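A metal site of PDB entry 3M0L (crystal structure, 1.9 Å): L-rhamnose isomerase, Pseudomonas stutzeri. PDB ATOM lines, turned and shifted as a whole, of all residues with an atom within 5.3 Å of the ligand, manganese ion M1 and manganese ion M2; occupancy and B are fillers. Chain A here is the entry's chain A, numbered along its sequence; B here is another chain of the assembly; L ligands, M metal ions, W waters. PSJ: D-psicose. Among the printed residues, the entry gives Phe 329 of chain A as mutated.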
ATOM      1  N   TRP A  57      -2.078 -14.229  -3.074  1.00  0.00           N
ATOM      2  CA  TRP A  57      -2.577 -14.411  -4.426  1.00  0.00           C
ATOM      3  C   TRP A  57      -1.936 -13.496  -5.462  1.00  0.00           C
ATOM      4  O   TRP A  57      -2.215 -13.594  -6.654  1.00  0.00           O
ATOM      5  CB  TRP A  57      -4.095 -14.256  -4.438  1.00  0.00           C
ATOM      6  CG  TRP A  57      -4.591 -12.899  -4.026  1.00  0.00           C
ATOM      7  CD1 TRP A  57      -4.812 -11.820  -4.835  1.00  0.00           C
ATOM      8  CD2 TRP A  57      -4.952 -12.483  -2.695  1.00  0.00           C
ATOM      9  NE1 TRP A  57      -5.279 -10.756  -4.092  1.00  0.00           N
ATOM     10  CE2 TRP A  57      -5.378 -11.145  -2.779  1.00  0.00           C
ATOM     11  CE3 TRP A  57      -4.938 -13.121  -1.451  1.00  0.00           C
ATOM     12  CZ2 TRP A  57      -5.790 -10.417  -1.655  1.00  0.00           C
ATOM     13  CZ3 TRP A  57      -5.364 -12.404  -0.329  1.00  0.00           C
ATOM     14  CH2 TRP A  57      -5.779 -11.065  -0.447  1.00  0.00           C
ATOM     15  N   HIS A 101      -5.548 -16.281   1.867  1.00  0.00           N
ATOM     16  CA  HIS A 101      -6.878 -16.471   1.304  1.00  0.00           C
ATOM     17  C   HIS A 101      -7.232 -17.944   1.450  1.00  0.00           C
ATOM     18  O   HIS A 101      -6.487 -18.821   1.004  1.00  0.00           O
ATOM     19  CB  HIS A 101      -6.888 -16.062  -0.166  1.00  0.00           C
ATOM     20  CG  HIS A 101      -8.142 -15.372  -0.587  1.00  0.00           C
ATOM     21  ND1 HIS A 101      -9.389 -15.966  -0.543  1.00  0.00           N
ATOM     22  CD2 HIS A 101      -8.355 -14.110  -1.048  1.00  0.00           C
ATOM     23  CE1 HIS A 101     -10.305 -15.109  -0.951  1.00  0.00           C
ATOM     24  NE2 HIS A 101      -9.708 -13.977  -1.258  1.00  0.00           N
ATOM     25  N   TRP A 104      -7.675 -21.211  -0.805  1.00  0.00           N
ATOM     26  CA  TRP A 104      -6.471 -21.236  -1.626  1.00  0.00           C
ATOM     27  C   TRP A 104      -5.207 -21.592  -0.839  1.00  0.00           C
ATOM     28  O   TRP A 104      -4.428 -22.442  -1.258  1.00  0.00           O
ATOM     29  CB  TRP A 104      -6.237 -19.883  -2.330  1.00  0.00           C
ATOM     30  CG  TRP A 104      -7.280 -19.486  -3.320  1.00  0.00           C
ATOM     31  CD1 TRP A 104      -8.176 -20.313  -3.953  1.00  0.00           C
ATOM     32  CD2 TRP A 104      -7.542 -18.163  -3.804  1.00  0.00           C
ATOM     33  NE1 TRP A 104      -8.974 -19.571  -4.792  1.00  0.00           N
ATOM     34  CE2 TRP A 104      -8.608 -18.250  -4.717  1.00  0.00           C
ATOM     35  CE3 TRP A 104      -6.971 -16.909  -3.540  1.00  0.00           C
ATOM     36  CZ2 TRP A 104      -9.123 -17.129  -5.386  1.00  0.00           C
ATOM     37  CZ3 TRP A 104      -7.490 -15.794  -4.202  1.00  0.00           C
ATOM     38  CH2 TRP A 104      -8.547 -15.913  -5.107  1.00  0.00           C
ATOM     39  N   ASN A 127      -8.680 -13.846   4.636  1.00  0.00           N
ATOM     40  CA  ASN A 127      -9.633 -13.570   3.578  1.00  0.00           C
ATOM     41  C   ASN A 127     -10.430 -14.842   3.312  1.00  0.00           C
ATOM     42  O   ASN A 127      -9.846 -15.894   3.055  1.00  0.00           O
ATOM     43  CB  ASN A 127      -8.908 -13.157   2.295  1.00  0.00           C
ATOM     44  CG  ASN A 127      -8.169 -11.837   2.442  1.00  0.00           C
ATOM     45  OD1 ASN A 127      -8.722 -10.767   2.194  1.00  0.00           O
ATOM     46  ND2 ASN A 127      -6.899 -11.909   2.843  1.00  0.00           N
ATOM     47  N   SER A 128     -11.749 -14.744   3.382  1.00  0.00           N
ATOM     48  CA  SER A 128     -12.609 -15.901   3.125  1.00  0.00           C
ATOM     49  C   SER A 128     -12.966 -15.979   1.643  1.00  0.00           C
ATOM     50  O   SER A 128     -12.861 -14.997   0.918  1.00  0.00           O
ATOM     51  CB  SER A 128     -13.895 -15.808   3.966  1.00  0.00           C
ATOM     52  OG  SER A 128     -14.577 -14.593   3.726  1.00  0.00           O
ATOM     53  N   PHE A 131     -17.050 -17.138  -3.070  1.00  0.00           N
ATOM     54  CA  PHE A 131     -17.380 -16.633  -4.400  1.00  0.00           C
ATOM     55  C   PHE A 131     -16.957 -17.661  -5.456  1.00  0.00           C
ATOM     56  O   PHE A 131     -16.943 -17.383  -6.653  1.00  0.00           O
ATOM     57  CB  PHE A 131     -16.682 -15.277  -4.646  1.00  0.00           C
ATOM     58  CG  PHE A 131     -15.194 -15.283  -4.416  1.00  0.00           C
ATOM     59  CD1 PHE A 131     -14.336 -15.847  -5.344  1.00  0.00           C
ATOM     60  CD2 PHE A 131     -14.654 -14.717  -3.274  1.00  0.00           C
ATOM     61  CE1 PHE A 131     -12.957 -15.846  -5.143  1.00  0.00           C
ATOM     62  CE2 PHE A 131     -13.278 -14.706  -3.052  1.00  0.00           C
ATOM     63  CZ  PHE A 131     -12.430 -15.275  -3.990  1.00  0.00           C
ATOM     64  N   TRP A 179     -15.230 -10.503   1.371  1.00  0.00           N
ATOM     65  CA  TRP A 179     -15.641  -9.973   0.082  1.00  0.00           C
ATOM     66  C   TRP A 179     -16.344 -11.131  -0.608  1.00  0.00           C
ATOM     67  O   TRP A 179     -15.797 -12.223  -0.683  1.00  0.00           O
ATOM     68  CB  TRP A 179     -14.463  -9.540  -0.794  1.00  0.00           C
ATOM     69  CG  TRP A 179     -14.958  -9.184  -2.178  1.00  0.00           C
ATOM     70  CD1 TRP A 179     -15.630  -8.050  -2.542  1.00  0.00           C
ATOM     71  CD2 TRP A 179     -14.919 -10.013  -3.343  1.00  0.00           C
ATOM     72  NE1 TRP A 179     -16.020  -8.133  -3.854  1.00  0.00           N
ATOM     73  CE2 TRP A 179     -15.598  -9.322  -4.373  1.00  0.00           C
ATOM     74  CE3 TRP A 179     -14.393 -11.288  -3.621  1.00  0.00           C
ATOM     75  CZ2 TRP A 179     -15.775  -9.856  -5.657  1.00  0.00           C
ATOM     76  CZ3 TRP A 179     -14.556 -11.813  -4.904  1.00  0.00           C
ATOM     77  CH2 TRP A 179     -15.237 -11.103  -5.907  1.00  0.00           C
ATOM     78  N   GLU A 219     -15.900  -5.726   2.473  1.00  0.00           N
ATOM     79  CA  GLU A 219     -15.376  -5.003   1.322  1.00  0.00           C
ATOM     80  C   GLU A 219     -16.407  -4.801   0.220  1.00  0.00           C
ATOM     81  O   GLU A 219     -16.903  -5.768  -0.362  1.00  0.00           O
ATOM     82  CB  GLU A 219     -14.154  -5.758   0.784  1.00  0.00           C
ATOM     83  CG  GLU A 219     -13.539  -5.168  -0.484  1.00  0.00           C
ATOM     84  CD  GLU A 219     -12.328  -5.938  -0.970  1.00  0.00           C
ATOM     85  OE1 GLU A 219     -12.064  -7.046  -0.433  1.00  0.00           O
ATOM     86  OE2 GLU A 219     -11.640  -5.458  -1.883  1.00  0.00           O
ATOM     87  N   LYS A 221     -17.959  -3.525  -3.526  1.00  0.00           N
ATOM     88  CA  LYS A 221     -17.537  -3.561  -4.921  1.00  0.00           C
ATOM     89  C   LYS A 221     -18.764  -3.300  -5.787  1.00  0.00           C
ATOM     90  O   LYS A 221     -19.790  -3.950  -5.633  1.00  0.00           O
ATOM     91  CB  LYS A 221     -16.942  -4.927  -5.270  1.00  0.00           C
ATOM     92  CG  LYS A 221     -16.230  -4.936  -6.618  1.00  0.00           C
ATOM     93  CD  LYS A 221     -15.637  -6.313  -6.935  1.00  0.00           C
ATOM     94  CE  LYS A 221     -14.809  -6.267  -8.205  1.00  0.00           C
ATOM     95  NZ  LYS A 221     -14.326  -7.619  -8.606  1.00  0.00           N
ATOM     96  N   GLU A 224     -18.964  -7.098 -10.706  1.00  0.00           N
ATOM     97  CA  GLU A 224     -18.040  -8.194 -11.010  1.00  0.00           C
ATOM     98  C   GLU A 224     -17.766  -8.976  -9.728  1.00  0.00           C
ATOM     99  O   GLU A 224     -17.128  -8.477  -8.800  1.00  0.00           O
ATOM    100  CB  GLU A 224     -16.705  -7.712 -11.596  1.00  0.00           C
ATOM    101  CG  GLU A 224     -15.825  -8.901 -12.036  1.00  0.00           C
ATOM    102  CD  GLU A 224     -14.369  -8.548 -12.266  1.00  0.00           C
ATOM    103  OE1 GLU A 224     -13.849  -7.649 -11.585  1.00  0.00           O
ATOM    104  OE2 GLU A 224     -13.724  -9.195 -13.131  1.00  0.00           O
ATOM    105  N   LEU A 252     -13.655  -1.840   4.480  1.00  0.00           N
ATOM    106  CA  LEU A 252     -12.400  -1.921   3.754  1.00  0.00           C
ATOM    107  C   LEU A 252     -12.628  -1.322   2.375  1.00  0.00           C
ATOM    108  O   LEU A 252     -13.593  -1.653   1.691  1.00  0.00           O
ATOM    109  CB  LEU A 252     -11.937  -3.377   3.661  1.00  0.00           C
ATOM    110  CG  LEU A 252     -10.527  -3.591   3.102  1.00  0.00           C
ATOM    111  CD1 LEU A 252      -9.908  -4.852   3.710  1.00  0.00           C
ATOM    112  CD2 LEU A 252     -10.595  -3.685   1.592  1.00  0.00           C
ATOM    113  N   ASP A 254     -11.289  -0.814  -1.416  1.00  0.00           N
ATOM    114  CA  ASP A 254     -10.412  -1.327  -2.460  1.00  0.00           C
ATOM    115  C   ASP A 254     -10.497  -0.266  -3.549  1.00  0.00           C
ATOM    116  O   ASP A 254     -11.551  -0.044  -4.128  1.00  0.00           O
ATOM    117  CB  ASP A 254     -10.905  -2.660  -2.986  1.00  0.00           C
ATOM    118  CG  ASP A 254      -9.961  -3.277  -4.002  1.00  0.00           C
ATOM    119  OD1 ASP A 254      -9.580  -2.570  -4.958  1.00  0.00           O
ATOM    120  OD2 ASP A 254      -9.608  -4.470  -3.850  1.00  0.00           O
ATOM    121  N   HIS A 257     -12.652  -0.575  -6.823  1.00  0.00           N
ATOM    122  CA  HIS A 257     -14.043  -1.036  -6.705  1.00  0.00           C
ATOM    123  C   HIS A 257     -15.130   0.044  -6.780  1.00  0.00           C
ATOM    124  O   HIS A 257     -16.256  -0.177  -6.333  1.00  0.00           O
ATOM    125  CB  HIS A 257     -14.225  -1.810  -5.400  1.00  0.00           C
ATOM    126  CG  HIS A 257     -13.500  -3.108  -5.350  1.00  0.00           C
ATOM    127  ND1 HIS A 257     -13.706  -4.041  -4.356  1.00  0.00           N
ATOM    128  CD2 HIS A 257     -12.581  -3.655  -6.177  1.00  0.00           C
ATOM    129  CE1 HIS A 257     -12.949  -5.100  -4.575  1.00  0.00           C
ATOM    130  NE2 HIS A 257     -12.261  -4.892  -5.678  1.00  0.00           N
ATOM    131  N   HIS A 281      -7.205  -1.715   0.320  1.00  0.00           N
ATOM    132  CA  HIS A 281      -6.741  -2.732  -0.609  1.00  0.00           C
ATOM    133  C   HIS A 281      -6.196  -1.848  -1.724  1.00  0.00           C
ATOM    134  O   HIS A 281      -6.966  -1.246  -2.487  1.00  0.00           O
ATOM    135  CB  HIS A 281      -7.885  -3.604  -1.128  1.00  0.00           C
ATOM    136  CG  HIS A 281      -8.056  -4.893  -0.383  1.00  0.00           C
ATOM    137  ND1 HIS A 281      -8.817  -5.938  -0.871  1.00  0.00           N
ATOM    138  CD2 HIS A 281      -7.564  -5.309   0.804  1.00  0.00           C
ATOM    139  CE1 HIS A 281      -8.786  -6.936   0.002  1.00  0.00           C
ATOM    140  NE2 HIS A 281      -8.037  -6.576   1.025  1.00  0.00           N
ATOM    141  N   ASP A 289     -12.137  -2.898 -12.234  1.00  0.00           N
ATOM    142  CA  ASP A 289     -11.330  -3.396 -11.124  1.00  0.00           C
ATOM    143  C   ASP A 289     -10.128  -4.085 -11.774  1.00  0.00           C
ATOM    144  O   ASP A 289      -9.952  -5.293 -11.664  1.00  0.00           O
ATOM    145  CB  ASP A 289     -12.139  -4.372 -10.283  1.00  0.00           C
ATOM    146  CG  ASP A 289     -11.350  -4.918  -9.095  1.00  0.00           C
ATOM    147  OD1 ASP A 289     -10.496  -4.174  -8.562  1.00  0.00           O
ATOM    148  OD2 ASP A 289     -11.600  -6.069  -8.689  1.00  0.00           O
ATOM    149  N   ASP A 291      -7.023  -4.104 -11.094  1.00  0.00           N
ATOM    150  CA  ASP A 291      -6.023  -4.681 -10.195  1.00  0.00           C
ATOM    151  C   ASP A 291      -4.586  -4.514 -10.673  1.00  0.00           C
ATOM    152  O   ASP A 291      -3.772  -5.430 -10.532  1.00  0.00           O
ATOM    153  CB  ASP A 291      -6.321  -6.152  -9.946  1.00  0.00           C
ATOM    154  CG  ASP A 291      -7.467  -6.348  -8.983  1.00  0.00           C
ATOM    155  OD1 ASP A 291      -7.512  -5.598  -7.991  1.00  0.00           O
ATOM    156  OD2 ASP A 291      -8.298  -7.257  -9.202  1.00  0.00           O
ATOM    157  N   ASP A 327      -3.813  -5.433  -3.008  1.00  0.00           N
ATOM    158  CA  ASP A 327      -4.703  -6.419  -3.620  1.00  0.00           C
ATOM    159  C   ASP A 327      -4.565  -6.217  -5.120  1.00  0.00           C
ATOM    160  O   ASP A 327      -5.263  -5.417  -5.722  1.00  0.00           O
ATOM    161  CB  ASP A 327      -6.161  -6.222  -3.210  1.00  0.00           C
ATOM    162  CG  ASP A 327      -7.076  -7.268  -3.841  1.00  0.00           C
ATOM    163  OD1 ASP A 327      -6.582  -8.048  -4.684  1.00  0.00           O
ATOM    164  OD2 ASP A 327      -8.273  -7.315  -3.508  1.00  0.00           O
ATOM    165  N   PHE A 329      -3.285  -8.214  -9.099  1.00  0.00           N
ATOM    166  CA  PHE A 329      -3.040  -9.412  -9.875  1.00  0.00           C
ATOM    167  C   PHE A 329      -2.033  -8.999 -10.932  1.00  0.00           C
ATOM    168  O   PHE A 329      -2.115  -7.906 -11.502  1.00  0.00           O
ATOM    169  CB  PHE A 329      -4.327  -9.940 -10.518  1.00  0.00           C
ATOM    170  CG  PHE A 329      -5.208 -10.701  -9.570  1.00  0.00           C
ATOM    171  CD1 PHE A 329      -6.259 -10.081  -8.914  1.00  0.00           C
ATOM    172  CD2 PHE A 329      -4.936 -12.034  -9.266  1.00  0.00           C
ATOM    173  CE1 PHE A 329      -7.045 -10.772  -7.983  1.00  0.00           C
ATOM    174  CE2 PHE A 329      -5.705 -12.738  -8.336  1.00  0.00           C
ATOM    175  CZ  PHE A 329      -6.756 -12.097  -7.691  1.00  0.00           C
ATOM    176  N   ARG B  65     -13.625 -14.134 -14.128  1.00  0.00           N
ATOM    177  CA  ARG B  65     -12.270 -14.487 -13.739  1.00  0.00           C
ATOM    178  C   ARG B  65     -12.259 -15.081 -12.327  1.00  0.00           C
ATOM    179  O   ARG B  65     -11.277 -15.696 -11.906  1.00  0.00           O
ATOM    180  CB  ARG B  65     -11.338 -13.276 -13.798  1.00  0.00           C
ATOM    181  CG  ARG B  65     -11.751 -12.122 -12.916  1.00  0.00           C
ATOM    182  CD  ARG B  65     -10.637 -11.079 -12.752  1.00  0.00           C
ATOM    183  NE  ARG B  65     -11.161  -9.882 -12.106  1.00  0.00           N
ATOM    184  CZ  ARG B  65     -10.470  -9.067 -11.323  1.00  0.00           C
ATOM    185  NH1 ARG B  65      -9.192  -9.296 -11.048  1.00  0.00           N
ATOM    186  NH2 ARG B  65     -11.083  -8.012 -10.793  1.00  0.00           N
ATOM    187  N   PHE B  66     -13.363 -14.912 -11.600  1.00  0.00           N
ATOM    188  CA  PHE B  66     -13.480 -15.433 -10.233  1.00  0.00           C
ATOM    189  C   PHE B  66     -14.011 -16.854 -10.133  1.00  0.00           C
ATOM    190  O   PHE B  66     -13.634 -17.604  -9.222  1.00  0.00           O
ATOM    191  CB  PHE B  66     -14.356 -14.515  -9.391  1.00  0.00           C
ATOM    192  CG  PHE B  66     -13.737 -13.193  -9.104  1.00  0.00           C
ATOM    193  CD1 PHE B  66     -12.685 -13.087  -8.198  1.00  0.00           C
ATOM    194  CD2 PHE B  66     -14.156 -12.046  -9.768  1.00  0.00           C
ATOM    195  CE1 PHE B  66     -12.063 -11.868  -7.959  1.00  0.00           C
ATOM    196  CE2 PHE B  66     -13.553 -10.829  -9.542  1.00  0.00           C
ATOM    197  CZ  PHE B  66     -12.493 -10.734  -8.638  1.00  0.00           C
HETATM  198  C1  PSJ L   1     -12.430  -9.013  -5.455  1.00  0.00           C
HETATM  199  O1  PSJ L   1     -12.671  -8.015  -6.433  1.00  0.00           O
HETATM  200  C2  PSJ L   1     -11.590  -8.435  -4.313  1.00  0.00           C
HETATM  201  O2  PSJ L   1     -10.914  -7.411  -4.494  1.00  0.00           O
HETATM  202  C3  PSJ L   1     -11.422  -9.255  -3.051  1.00  0.00           C
HETATM  203  O3  PSJ L   1     -10.594  -8.554  -2.125  1.00  0.00           O
HETATM  204  C4  PSJ L   1     -10.785 -10.612  -3.384  1.00  0.00           C
HETATM  205  O4  PSJ L   1     -10.890 -11.489  -2.263  1.00  0.00           O
HETATM  206  C5  PSJ L   1      -9.317 -10.451  -3.793  1.00  0.00           C
HETATM  207  O5  PSJ L   1      -9.213  -9.541  -4.875  1.00  0.00           O
HETATM  208  C6  PSJ L   1      -8.743 -11.797  -4.194  1.00  0.00           C
HETATM  209  O6  PSJ L   1      -9.369 -12.246  -5.393  1.00  0.00           O
HETATM  210 MN    MN M   1      -9.803  -6.249  -2.635  1.00  0.00          MN
HETATM  211 MN    MN M   2     -11.248  -6.565  -6.571  1.00  0.00          MN
HETATM  212  O   HOH W   1      -9.938  -8.153  -7.233  1.00  0.00           O
HETATM  213  O   HOH W   2      -9.652  -5.482  -6.750  1.00  0.00           O
HETATM  214  O   HOH W   3     -10.958 -10.508   0.399  1.00  0.00           O
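NZ of Lys 221 sits close to O1 of the ligand (2.8 Å).
O4 of the ligand lies within hydrogen-bond range of NE2 of His 101.
The side-chain amino group of Lys 221 lies within salt-bridge range of the side-chain carboxylate of Glu 224, at 3.0 Å.
The side-chain carboxylate of Asp 327 lies within hydrogen-bond range of the indole nitrogen of Trp 57 (3.1 Å).
OD2 of Asp 289 sits close to NZ of Lys 221, at 3.1 Å.
The guanidinium group (NH2) of Arg 65 of chain B sits at hydrogen-bond distance from the backbone carbonyl oxygen (O) of Asp 289, at 3.1 Å.
The backbone carbonyl oxygen (O) of Asp 291 lies within hydrogen-bond range of the backbone NH (N) of Phe 329 (3.2 Å).
Trp 57 touches the ligand (NE1 to C6, 3.6 Å).
Trp 104 touches the ligand.
Trp 179 touches the ligand (CE2 to C1, 3.4 Å).
Phe 329 touches the ligand (CZ to O6, 3.5 Å).
Phe 66 of chain B touches the ligand.
Hydrophobic or aromatic side chains within 4 Å of the ligand: Trp 57, His 101, Trp 104, Trp 179, His 257, His 281, Phe 329 and Phe 66 of chain B.
13 residues have an atom within 4 Å of the ligand: Trp 57, His 101, Trp 104, Trp 179, Glu 219, Lys 221, Asp 254, His 257, His 281, Asp 289, Asp 327, Phe 329 and Phe 66 of chain B.
The nearest printed residue that does not touch the ligand is Phe 131 (4.1 Å).
Of the 20 residues printed, 5 come within 4 Å of manganese ion M1.
Residues that only touch manganese ion M2: Lys 221 (3.8 Å).
Along chain A the residues within 4 Å of manganese ion M2 span positions 221 to 289.
Manganese ion M1 is bound by a ring nitrogen (ND1) of His 281, the side-chain carboxylate of Asp 327, the side-chain carboxylate of Glu 219, the side-chain carboxylate of Asp 254, an oxygen (O2) of the ligand and an oxygen (O3) of the ligand.
Manganese ion M2 is bound by water W2 (1.9 Å), O1 of the ligand (2.0 Å), NE2 of His 257 (2.2 Å), water W1 (2.2 Å), OD2 of Asp 289 (2.2 Å) and O2 of the ligand (2.3 Å).
Water W1 lies within hydrogen-bond range of OD2 of Asp 291 (2.7 Å) and O5 of the ligand (2.8 Å).
Water W2 lies within hydrogen-bond range of the side-chain carboxylate of Asp 291 (2.5 Å) and the side-chain carboxylate of Asp 254 (3.4 Å).
Water W3 bridges O4 of the ligand (2.8 Å) and OD1 of Asn 127 (2.9 Å).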
